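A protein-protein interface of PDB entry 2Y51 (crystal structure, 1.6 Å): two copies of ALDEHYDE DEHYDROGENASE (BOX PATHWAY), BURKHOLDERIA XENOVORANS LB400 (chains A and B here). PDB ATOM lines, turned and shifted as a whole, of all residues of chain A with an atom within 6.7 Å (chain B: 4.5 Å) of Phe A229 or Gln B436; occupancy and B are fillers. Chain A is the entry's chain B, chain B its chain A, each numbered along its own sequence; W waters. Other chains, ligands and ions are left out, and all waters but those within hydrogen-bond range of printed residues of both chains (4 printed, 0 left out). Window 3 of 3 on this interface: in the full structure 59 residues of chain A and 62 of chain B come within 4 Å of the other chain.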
ATOM      1  N   ARG A  53     -14.677 -18.746  -2.906  1.00  0.00           N
ATOM      2  CA  ARG A  53     -15.759 -18.096  -2.101  1.00  0.00           C
ATOM      3  C   ARG A  53     -15.251 -16.925  -1.292  1.00  0.00           C
ATOM      4  O   ARG A  53     -15.882 -15.818  -1.315  1.00  0.00           O
ATOM      5  CB  ARG A  53     -16.413 -19.084  -1.124  1.00  0.00           C
ATOM      6  CG  ARG A  53     -17.707 -18.495  -0.455  1.00  0.00           C
ATOM      7  CD  ARG A  53     -18.376 -19.556   0.373  1.00  0.00           C
ATOM      8  NE  ARG A  53     -18.773 -20.839  -0.254  1.00  0.00           N
ATOM      9  CZ  ARG A  53     -18.152 -21.994  -0.065  1.00  0.00           C
ATOM     10  NH1 ARG A  53     -17.033 -22.035   0.683  1.00  0.00           N
ATOM     11  NH2 ARG A  53     -18.586 -23.128  -0.647  1.00  0.00           N
ATOM     12  N   THR A 151     -24.877 -12.621  -3.553  1.00  0.00           N
ATOM     13  CA  THR A 151     -24.799 -13.722  -2.569  1.00  0.00           C
ATOM     14  C   THR A 151     -23.313 -13.958  -2.240  1.00  0.00           C
ATOM     15  O   THR A 151     -22.470 -13.929  -3.126  1.00  0.00           O
ATOM     16  CB  THR A 151     -25.493 -15.007  -3.049  1.00  0.00           C
ATOM     17  OG1 THR A 151     -25.593 -15.914  -1.907  1.00  0.00           O
ATOM     18  CG2 THR A 151     -24.747 -15.719  -4.216  1.00  0.00           C
ATOM     19  N   ARG A 152     -23.041 -14.122  -0.944  1.00  0.00           N
ATOM     20  CA  ARG A 152     -21.728 -14.386  -0.418  1.00  0.00           C
ATOM     21  C   ARG A 152     -21.423 -15.888  -0.574  1.00  0.00           C
ATOM     22  O   ARG A 152     -21.335 -16.644   0.382  1.00  0.00           O
ATOM     23  CB  ARG A 152     -21.644 -13.951   1.058  1.00  0.00           C
ATOM     24  CG  ARG A 152     -21.414 -12.459   1.158  1.00  0.00           C
ATOM     25  CD  ARG A 152     -21.281 -12.053   2.629  1.00  0.00           C
ATOM     26  NE  ARG A 152     -21.261 -10.592   2.675  1.00  0.00           N
ATOM     27  CZ  ARG A 152     -20.294  -9.877   3.212  1.00  0.00           C
ATOM     28  NH1 ARG A 152     -19.229 -10.494   3.736  1.00  0.00           N
ATOM     29  NH2 ARG A 152     -20.410  -8.561   3.196  1.00  0.00           N
ATOM     30  N   GLY A 153     -21.322 -16.322  -1.802  1.00  0.00           N
ATOM     31  CA  GLY A 153     -21.019 -17.737  -2.082  1.00  0.00           C
ATOM     32  C   GLY A 153     -20.339 -17.853  -3.420  1.00  0.00           C
ATOM     33  O   GLY A 153     -19.796 -16.875  -3.956  1.00  0.00           O
ATOM     34  N   VAL A 154     -20.296 -19.081  -3.906  1.00  0.00           N
ATOM     35  CA  VAL A 154     -19.723 -19.399  -5.241  1.00  0.00           C
ATOM     36  C   VAL A 154     -20.862 -19.894  -6.156  1.00  0.00           C
ATOM     37  O   VAL A 154     -21.930 -20.271  -5.676  1.00  0.00           O
ATOM     38  CB  VAL A 154     -18.645 -20.535  -5.216  1.00  0.00           C
ATOM     39  CG1 VAL A 154     -17.545 -20.067  -4.415  1.00  0.00           C
ATOM     40  CG2 VAL A 154     -19.305 -21.849  -4.713  1.00  0.00           C
ATOM     41  N   VAL A 180     -20.363 -12.590  -8.292  1.00  0.00           N
ATOM     42  CA  VAL A 180     -20.266 -13.959  -7.725  1.00  0.00           C
ATOM     43  C   VAL A 180     -19.203 -14.822  -8.467  1.00  0.00           C
ATOM     44  O   VAL A 180     -19.205 -14.977  -9.694  1.00  0.00           O
ATOM     45  CB  VAL A 180     -21.693 -14.695  -7.728  1.00  0.00           C
ATOM     46  CG1 VAL A 180     -21.541 -16.125  -7.315  1.00  0.00           C
ATOM     47  CG2 VAL A 180     -22.739 -13.912  -6.871  1.00  0.00           C
ATOM     48  N   ILE A 226     -20.488 -27.582  -1.462  1.00  0.00           N
ATOM     49  CA  ILE A 226     -21.493 -26.481  -1.605  1.00  0.00           C
ATOM     50  C   ILE A 226     -22.132 -26.119  -0.267  1.00  0.00           C
ATOM     51  O   ILE A 226     -22.461 -27.006   0.496  1.00  0.00           O
ATOM     52  CB  ILE A 226     -22.575 -26.911  -2.649  1.00  0.00           C
ATOM     53  CG1 ILE A 226     -21.935 -26.914  -4.034  1.00  0.00           C
ATOM     54  CG2 ILE A 226     -23.901 -26.081  -2.574  1.00  0.00           C
ATOM     55  CD1 ILE A 226     -21.587 -25.480  -4.550  1.00  0.00           C
ATOM     56  N   ARG A 227     -22.276 -24.831   0.018  1.00  0.00           N
ATOM     57  CA  ARG A 227     -22.855 -24.355   1.284  1.00  0.00           C
ATOM     58  C   ARG A 227     -24.073 -23.453   1.002  1.00  0.00           C
ATOM     59  O   ARG A 227     -24.429 -23.236  -0.124  1.00  0.00           O
ATOM     60  CB  ARG A 227     -21.823 -23.552   2.078  1.00  0.00           C
ATOM     61  CG  ARG A 227     -20.641 -24.468   2.576  1.00  0.00           C
ATOM     62  CD  ARG A 227     -19.623 -23.486   3.191  1.00  0.00           C
ATOM     63  NE  ARG A 227     -18.402 -23.913   3.915  1.00  0.00           N
ATOM     64  CZ  ARG A 227     -17.971 -25.146   4.163  1.00  0.00           C
ATOM     65  NH1 ARG A 227     -18.659 -26.239   3.722  1.00  0.00           N
ATOM     66  NH2 ARG A 227     -16.821 -25.275   4.873  1.00  0.00           N
ATOM     67  N   SER A 228     -24.698 -22.979   2.074  1.00  0.00           N
ATOM     68  CA  SER A 228     -26.072 -22.437   1.910  1.00  0.00           C
ATOM     69  C   SER A 228     -26.203 -21.170   1.103  1.00  0.00           C
ATOM     70  O   SER A 228     -27.346 -20.857   0.679  1.00  0.00           O
ATOM     71  CB  SER A 228     -26.722 -22.246   3.272  1.00  0.00           C
ATOM     72  OG  SER A 228     -26.017 -21.226   3.935  1.00  0.00           O
ATOM     73  N   PHE A 229     -25.127 -20.428   0.944  1.00  0.00           N
ATOM     74  CA  PHE A 229     -25.238 -19.140   0.193  1.00  0.00           C
ATOM     75  C   PHE A 229     -24.690 -19.334  -1.225  1.00  0.00           C
ATOM     76  O   PHE A 229     -24.512 -18.361  -1.982  1.00  0.00           O
ATOM     77  CB  PHE A 229     -24.551 -18.034   0.937  1.00  0.00           C
ATOM     78  CG  PHE A 229     -25.271 -17.609   2.207  1.00  0.00           C
ATOM     79  CD1 PHE A 229     -25.124 -18.357   3.387  1.00  0.00           C
ATOM     80  CD2 PHE A 229     -26.141 -16.497   2.185  1.00  0.00           C
ATOM     81  CE1 PHE A 229     -25.807 -18.024   4.568  1.00  0.00           C
ATOM     82  CE2 PHE A 229     -26.834 -16.112   3.392  1.00  0.00           C
ATOM     83  CZ  PHE A 229     -26.663 -16.946   4.583  1.00  0.00           C
ATOM     84  N   ASP A 230     -24.361 -20.568  -1.571  1.00  0.00           N
ATOM     85  CA  ASP A 230     -23.820 -20.862  -2.901  1.00  0.00           C
ATOM     86  C   ASP A 230     -24.966 -21.104  -3.860  1.00  0.00           C
ATOM     87  O   ASP A 230     -26.108 -21.402  -3.446  1.00  0.00           O
ATOM     88  CB  ASP A 230     -22.986 -22.140  -2.855  1.00  0.00           C
ATOM     89  CG  ASP A 230     -21.702 -21.964  -2.075  1.00  0.00           C
ATOM     90  OD1 ASP A 230     -21.252 -20.840  -1.852  1.00  0.00           O
ATOM     91  OD2 ASP A 230     -21.102 -23.025  -1.744  1.00  0.00           O
ATOM     92  N   VAL A 231     -24.675 -21.062  -5.166  1.00  0.00           N
ATOM     93  CA  VAL A 231     -25.702 -21.452  -6.126  1.00  0.00           C
ATOM     94  C   VAL A 231     -25.170 -22.443  -7.138  1.00  0.00           C
ATOM     95  O   VAL A 231     -23.953 -22.494  -7.424  1.00  0.00           O
ATOM     96  CB  VAL A 231     -26.251 -20.170  -6.897  1.00  0.00           C
ATOM     97  CG1 VAL A 231     -26.738 -19.163  -5.876  1.00  0.00           C
ATOM     98  CG2 VAL A 231     -25.187 -19.625  -7.879  1.00  0.00           C
ATOM     99  N   ARG A 253     -28.695 -28.185   3.323  1.00  0.00           N
ATOM    100  CA  ARG A 253     -28.152 -26.807   3.287  1.00  0.00           C
ATOM    101  C   ARG A 253     -28.900 -25.715   2.530  1.00  0.00           C
ATOM    102  O   ARG A 253     -28.659 -24.565   2.758  1.00  0.00           O
ATOM    103  CB  ARG A 253     -26.647 -26.797   2.995  1.00  0.00           C
ATOM    104  CG  ARG A 253     -26.005 -27.809   3.973  1.00  0.00           C
ATOM    105  CD  ARG A 253     -24.456 -27.911   4.015  1.00  0.00           C
ATOM    106  NE  ARG A 253     -23.908 -28.353   2.735  1.00  0.00           N
ATOM    107  CZ  ARG A 253     -23.575 -29.613   2.426  1.00  0.00           C
ATOM    108  NH1 ARG A 253     -23.729 -30.596   3.308  1.00  0.00           N
ATOM    109  NH2 ARG A 253     -23.068 -29.888   1.200  1.00  0.00           N
ATOM    110  N   GLY A 254     -29.829 -26.136   1.671  1.00  0.00           N
ATOM    111  CA  GLY A 254     -30.752 -25.214   1.037  1.00  0.00           C
ATOM    112  C   GLY A 254     -30.127 -24.320  -0.015  1.00  0.00           C
ATOM    113  O   GLY A 254     -30.694 -23.266  -0.323  1.00  0.00           O
ATOM    114  N   ALA A 255     -28.951 -24.691  -0.516  1.00  0.00           N
ATOM    115  CA  ALA A 255     -28.316 -23.949  -1.598  1.00  0.00           C
ATOM    116  C   ALA A 255     -29.282 -23.852  -2.799  1.00  0.00           C
ATOM    117  O   ALA A 255     -29.961 -24.800  -3.134  1.00  0.00           O
ATOM    118  CB  ALA A 255     -27.013 -24.646  -2.089  1.00  0.00           C
ATOM    119  N   ARG A 256     -29.288 -22.725  -3.477  1.00  0.00           N
ATOM    120  CA  ARG A 256     -30.146 -22.566  -4.636  1.00  0.00           C
ATOM    121  C   ARG A 256     -29.666 -23.357  -5.845  1.00  0.00           C
ATOM    122  O   ARG A 256     -28.489 -23.445  -6.146  1.00  0.00           O
ATOM    123  CB  ARG A 256     -30.108 -21.101  -5.137  1.00  0.00           C
ATOM    124  CG  ARG A 256     -30.547 -20.108  -4.334  1.00  0.00           C
ATOM    125  CD  ARG A 256     -31.050 -19.007  -5.339  1.00  0.00           C
ATOM    126  NE  ARG A 256     -31.743 -18.070  -4.499  1.00  0.00           N
ATOM    127  CZ  ARG A 256     -31.529 -16.761  -4.479  1.00  0.00           C
ATOM    128  NH1 ARG A 256     -30.577 -16.231  -5.224  1.00  0.00           N
ATOM    129  NH2 ARG A 256     -32.234 -16.047  -3.616  1.00  0.00           N
ATOM    130  N   ARG A 511     -29.305 -11.861  -3.191  1.00  0.00           N
ATOM    131  CA  ARG A 511     -30.274 -12.034  -2.115  1.00  0.00           C
ATOM    132  C   ARG A 511     -31.157 -10.812  -2.091  1.00  0.00           C
ATOM    133  O   ARG A 511     -30.641  -9.689  -2.175  1.00  0.00           O
ATOM    134  CB  ARG A 511     -29.546 -12.118  -0.773  1.00  0.00           C
ATOM    135  CG  ARG A 511     -28.579 -13.241  -0.705  1.00  0.00           C
ATOM    136  CD  ARG A 511     -29.414 -14.589  -0.685  1.00  0.00           C
ATOM    137  NE  ARG A 511     -28.557 -15.630  -1.107  1.00  0.00           N
ATOM    138  CZ  ARG A 511     -28.883 -16.883  -1.235  1.00  0.00           C
ATOM    139  NH1 ARG A 511     -30.119 -17.331  -0.966  1.00  0.00           N
ATOM    140  NH2 ARG A 511     -27.962 -17.661  -1.674  1.00  0.00           N
ATOM    141  N   ARG B 433     -24.614 -12.035  11.240  1.00  0.00           N
ATOM    142  CA  ARG B 433     -24.316 -13.014  10.204  1.00  0.00           C
ATOM    143  C   ARG B 433     -24.019 -14.408  10.827  1.00  0.00           C
ATOM    144  O   ARG B 433     -24.191 -15.413  10.121  1.00  0.00           O
ATOM    145  CB  ARG B 433     -23.100 -12.546   9.394  1.00  0.00           C
ATOM    146  CG  ARG B 433     -23.320 -11.458   8.388  1.00  0.00           C
ATOM    147  CD  ARG B 433     -21.996 -11.243   7.674  1.00  0.00           C
ATOM    148  NE  ARG B 433     -22.142 -10.055   6.877  1.00  0.00           N
ATOM    149  CZ  ARG B 433     -21.245  -9.079   6.757  1.00  0.00           C
ATOM    150  NH1 ARG B 433     -20.073  -9.115   7.433  1.00  0.00           N
ATOM    151  NH2 ARG B 433     -21.549  -8.025   5.981  1.00  0.00           N
ATOM    152  N   ARG B 434     -23.510 -14.480  12.082  1.00  0.00           N
ATOM    153  CA  ARG B 434     -23.224 -15.813  12.663  1.00  0.00           C
ATOM    154  C   ARG B 434     -24.507 -16.643  12.856  1.00  0.00           C
ATOM    155  O   ARG B 434     -24.474 -17.855  13.099  1.00  0.00           O
ATOM    156  CB  ARG B 434     -22.507 -15.704  14.015  1.00  0.00           C
ATOM    157  CG  ARG B 434     -21.146 -15.044  13.925  1.00  0.00           C
ATOM    158  CD  ARG B 434     -20.107 -16.070  13.642  1.00  0.00           C
ATOM    159  NE  ARG B 434     -20.147 -17.201  14.594  1.00  0.00           N
ATOM    160  CZ  ARG B 434     -19.404 -17.311  15.717  1.00  0.00           C
ATOM    161  NH1 ARG B 434     -18.555 -16.351  16.090  1.00  0.00           N
ATOM    162  NH2 ARG B 434     -19.531 -18.387  16.488  1.00  0.00           N
ATOM    163  N   GLY B 435     -25.653 -15.976  12.761  1.00  0.00           N
ATOM    164  CA  GLY B 435     -26.933 -16.639  12.801  1.00  0.00           C
ATOM    165  C   GLY B 435     -27.213 -17.415  11.536  1.00  0.00           C
ATOM    166  O   GLY B 435     -28.193 -18.140  11.498  1.00  0.00           O
ATOM    167  N   GLN B 436     -26.340 -17.314  10.517  1.00  0.00           N
ATOM    168  CA  GLN B 436     -26.365 -18.160   9.294  1.00  0.00           C
ATOM    169  C   GLN B 436     -27.562 -17.840   8.368  1.00  0.00           C
ATOM    170  O   GLN B 436     -27.950 -18.673   7.528  1.00  0.00           O
ATOM    171  CB  GLN B 436     -26.328 -19.702   9.642  1.00  0.00           C
ATOM    172  CG  GLN B 436     -25.208 -20.075  10.583  1.00  0.00           C
ATOM    173  CD  GLN B 436     -23.950 -20.233   9.881  1.00  0.00           C
ATOM    174  OE1 GLN B 436     -23.701 -21.294   9.263  1.00  0.00           O
ATOM    175  NE2 GLN B 436     -23.092 -19.215   9.970  1.00  0.00           N
ATOM    176  N   GLY B 437     -28.125 -16.658   8.508  1.00  0.00           N
ATOM    177  CA  GLY B 437     -29.230 -16.207   7.594  1.00  0.00           C
ATOM    178  C   GLY B 437     -30.528 -16.161   8.384  1.00  0.00           C
ATOM    179  O   GLY B 437     -30.973 -17.187   8.973  1.00  0.00           O
ATOM    180  N   ASP B 460     -27.597  -8.877   2.705  1.00  0.00           N
ATOM    181  CA  ASP B 460     -27.329 -10.145   2.031  1.00  0.00           C
ATOM    182  C   ASP B 460     -27.480 -11.342   2.993  1.00  0.00           C
ATOM    183  O   ASP B 460     -27.363 -12.495   2.538  1.00  0.00           O
ATOM    184  CB  ASP B 460     -25.941 -10.110   1.330  1.00  0.00           C
ATOM    185  CG  ASP B 460     -24.727  -9.996   2.333  1.00  0.00           C
ATOM    186  OD1 ASP B 460     -24.862 -10.349   3.524  1.00  0.00           O
ATOM    187  OD2 ASP B 460     -23.589  -9.523   1.923  1.00  0.00           O
ATOM    188  N   SER B 461     -27.787 -11.088   4.266  1.00  0.00           N
ATOM    189  CA  SER B 461     -28.013 -12.207   5.190  1.00  0.00           C
ATOM    190  C   SER B 461     -29.379 -12.113   5.856  1.00  0.00           C
ATOM    191  O   SER B 461     -29.727 -12.978   6.630  1.00  0.00           O
ATOM    192  CB  SER B 461     -26.887 -12.236   6.201  1.00  0.00           C
ATOM    193  OG  SER B 461     -26.896 -11.018   6.916  1.00  0.00           O
ATOM    194  N   PRO B 491     -32.452 -15.950   3.926  1.00  0.00           N
ATOM    195  CA  PRO B 491     -31.536 -16.954   3.353  1.00  0.00           C
ATOM    196  C   PRO B 491     -31.001 -17.903   4.407  1.00  0.00           C
ATOM    197  O   PRO B 491     -31.192 -17.722   5.647  1.00  0.00           O
ATOM    198  CB  PRO B 491     -30.385 -16.084   2.810  1.00  0.00           C
ATOM    199  CG  PRO B 491     -30.345 -14.929   3.912  1.00  0.00           C
ATOM    200  CD  PRO B 491     -31.826 -14.607   4.014  1.00  0.00           C
ATOM    201  N   GLY B 492     -30.368 -18.970   3.942  1.00  0.00           N
ATOM    202  CA  GLY B 492     -29.634 -19.826   4.856  1.00  0.00           C
ATOM    203  C   GLY B 492     -30.531 -20.542   5.840  1.00  0.00           C
ATOM    204  O   GLY B 492     -31.511 -21.138   5.454  1.00  0.00           O
ATOM    205  N   ARG B 493     -30.190 -20.469   7.138  1.00  0.00           N
ATOM    206  CA  ARG B 493     -30.946 -21.163   8.178  1.00  0.00           C
ATOM    207  C   ARG B 493     -32.459 -20.853   8.131  1.00  0.00           C
ATOM    208  O   ARG B 493     -33.312 -21.734   8.398  1.00  0.00           O
ATOM    209  CB  ARG B 493     -30.334 -20.836   9.544  1.00  0.00           C
ATOM    210  CG  ARG B 493     -31.002 -21.413  10.790  1.00  0.00           C
ATOM    211  CD  ARG B 493     -30.085 -21.145  12.017  1.00  0.00           C
ATOM    212  NE  ARG B 493     -28.895 -22.023  12.021  1.00  0.00           N
ATOM    213  CZ  ARG B 493     -27.710 -21.719  12.574  1.00  0.00           C
ATOM    214  NH1 ARG B 493     -27.502 -20.549  13.156  1.00  0.00           N
ATOM    215  NH2 ARG B 493     -26.705 -22.583  12.529  1.00  0.00           N
HETATM  216  O   HOH W   1     -25.029 -13.669   1.299  1.00  0.00           O
HETATM  217  O   HOH W   2     -29.993 -20.409   1.497  1.00  0.00           O
HETATM  218  O   HOH W   3     -26.706 -20.978   6.322  1.00  0.00           O
HETATM  219  O   HOH W   4     -22.680  -6.947   2.532  1.00  0.00           O
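The side-chain hydroxyl (OG1) of Thr A151 lies within hydrogen-bond range of the backbone carbonyl oxygen (O) of Phe A229. The side-chain hydroxyl of Thr A151 lies within hydrogen-bond range of the guanidinium group of Arg A511 (3.0 Å). O of Gln B436 lies within hydrogen-bond range of N of Arg B493.
The guanidinium group of Arg B433 lies close to the guanidinium group of Arg A152, 3.1 Å away. NE of Arg A152 is in salt-bridge range of OD2 of Asp B460 (2.7 Å).
No position is printed for both chains.
Water W3 bridges OG of Ser A228 (2.5 Å) and O of Gln B436 (2.9 Å). Water W4 bridges the side-chain carboxylate of Asp B460 (2.8 Å) and the guanidinium group of Arg A152 (2.9 Å). Water W2 lies within hydrogen-bond range of the backbone carbonyl oxygen of Ser A228, the backbone NH of Gly B492 and the backbone carbonyl oxygen of Gly A254. Water W1 lies within hydrogen-bond range of O of Asp B460 (2.9 Å) and N of Arg A152 (3.0 Å).
Among the printed residues, pairs that only touch across the chains: Ser A228 with Gly B492, Phe A229 with Gln B436, Phe A229 with Asp B460, Phe A229 with Pro B491, Arg A511 with Asp B460 and Arg A511 with Pro B491.
Hydrophobic or aromatic side chains of chain B that line the printed part of chain A: Pro B491. Along chain A the printed residues that touch a printed residue of chain B span positions 152 to 511. Among the printed residues, 8 pairs touch across the chains. Among the printed residues, Asp or Glu carboxylates within 4 Å of a Lys or Arg side-chain nitrogen of the other chain: Arg A152 with Asp B460.
Of the printed residues of chain B, Ser A228 touches Gly B492. Phe A229 touches just these residues of chain B: Gln B436 (3.6 Å), Asp B460 (3.8 Å) and Pro B491 (3.6 Å). Printed residues of chain B within 4 Å of Arg A511: Asp B460 and Pro B491. Of the printed residues of chain A, Arg B433 touches Arg A152. Gly B435 touches none of the printed residues of chain A. Of the printed residues of chain A, Gln B436 touches Phe A229 (3.6 Å). Printed residues of chain A within 4 Å of Asp B460: Arg A152 (2.7 Å), Phe A229 (3.8 Å) and Arg A511 (3.5 Å). Printed residues of chain A within 4 Å of Pro B491: Phe A229 (3.6 Å) and Arg A511 (3.9 Å). Arg B493 touches none of the printed residues of chain A. The nearest residue of chain A that does not touch Gln B436 is Ser A228 (4.8 Å). The nearest printed residue of chain A that does not touch Pro B491 is Ser A228 (6.0 Å).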
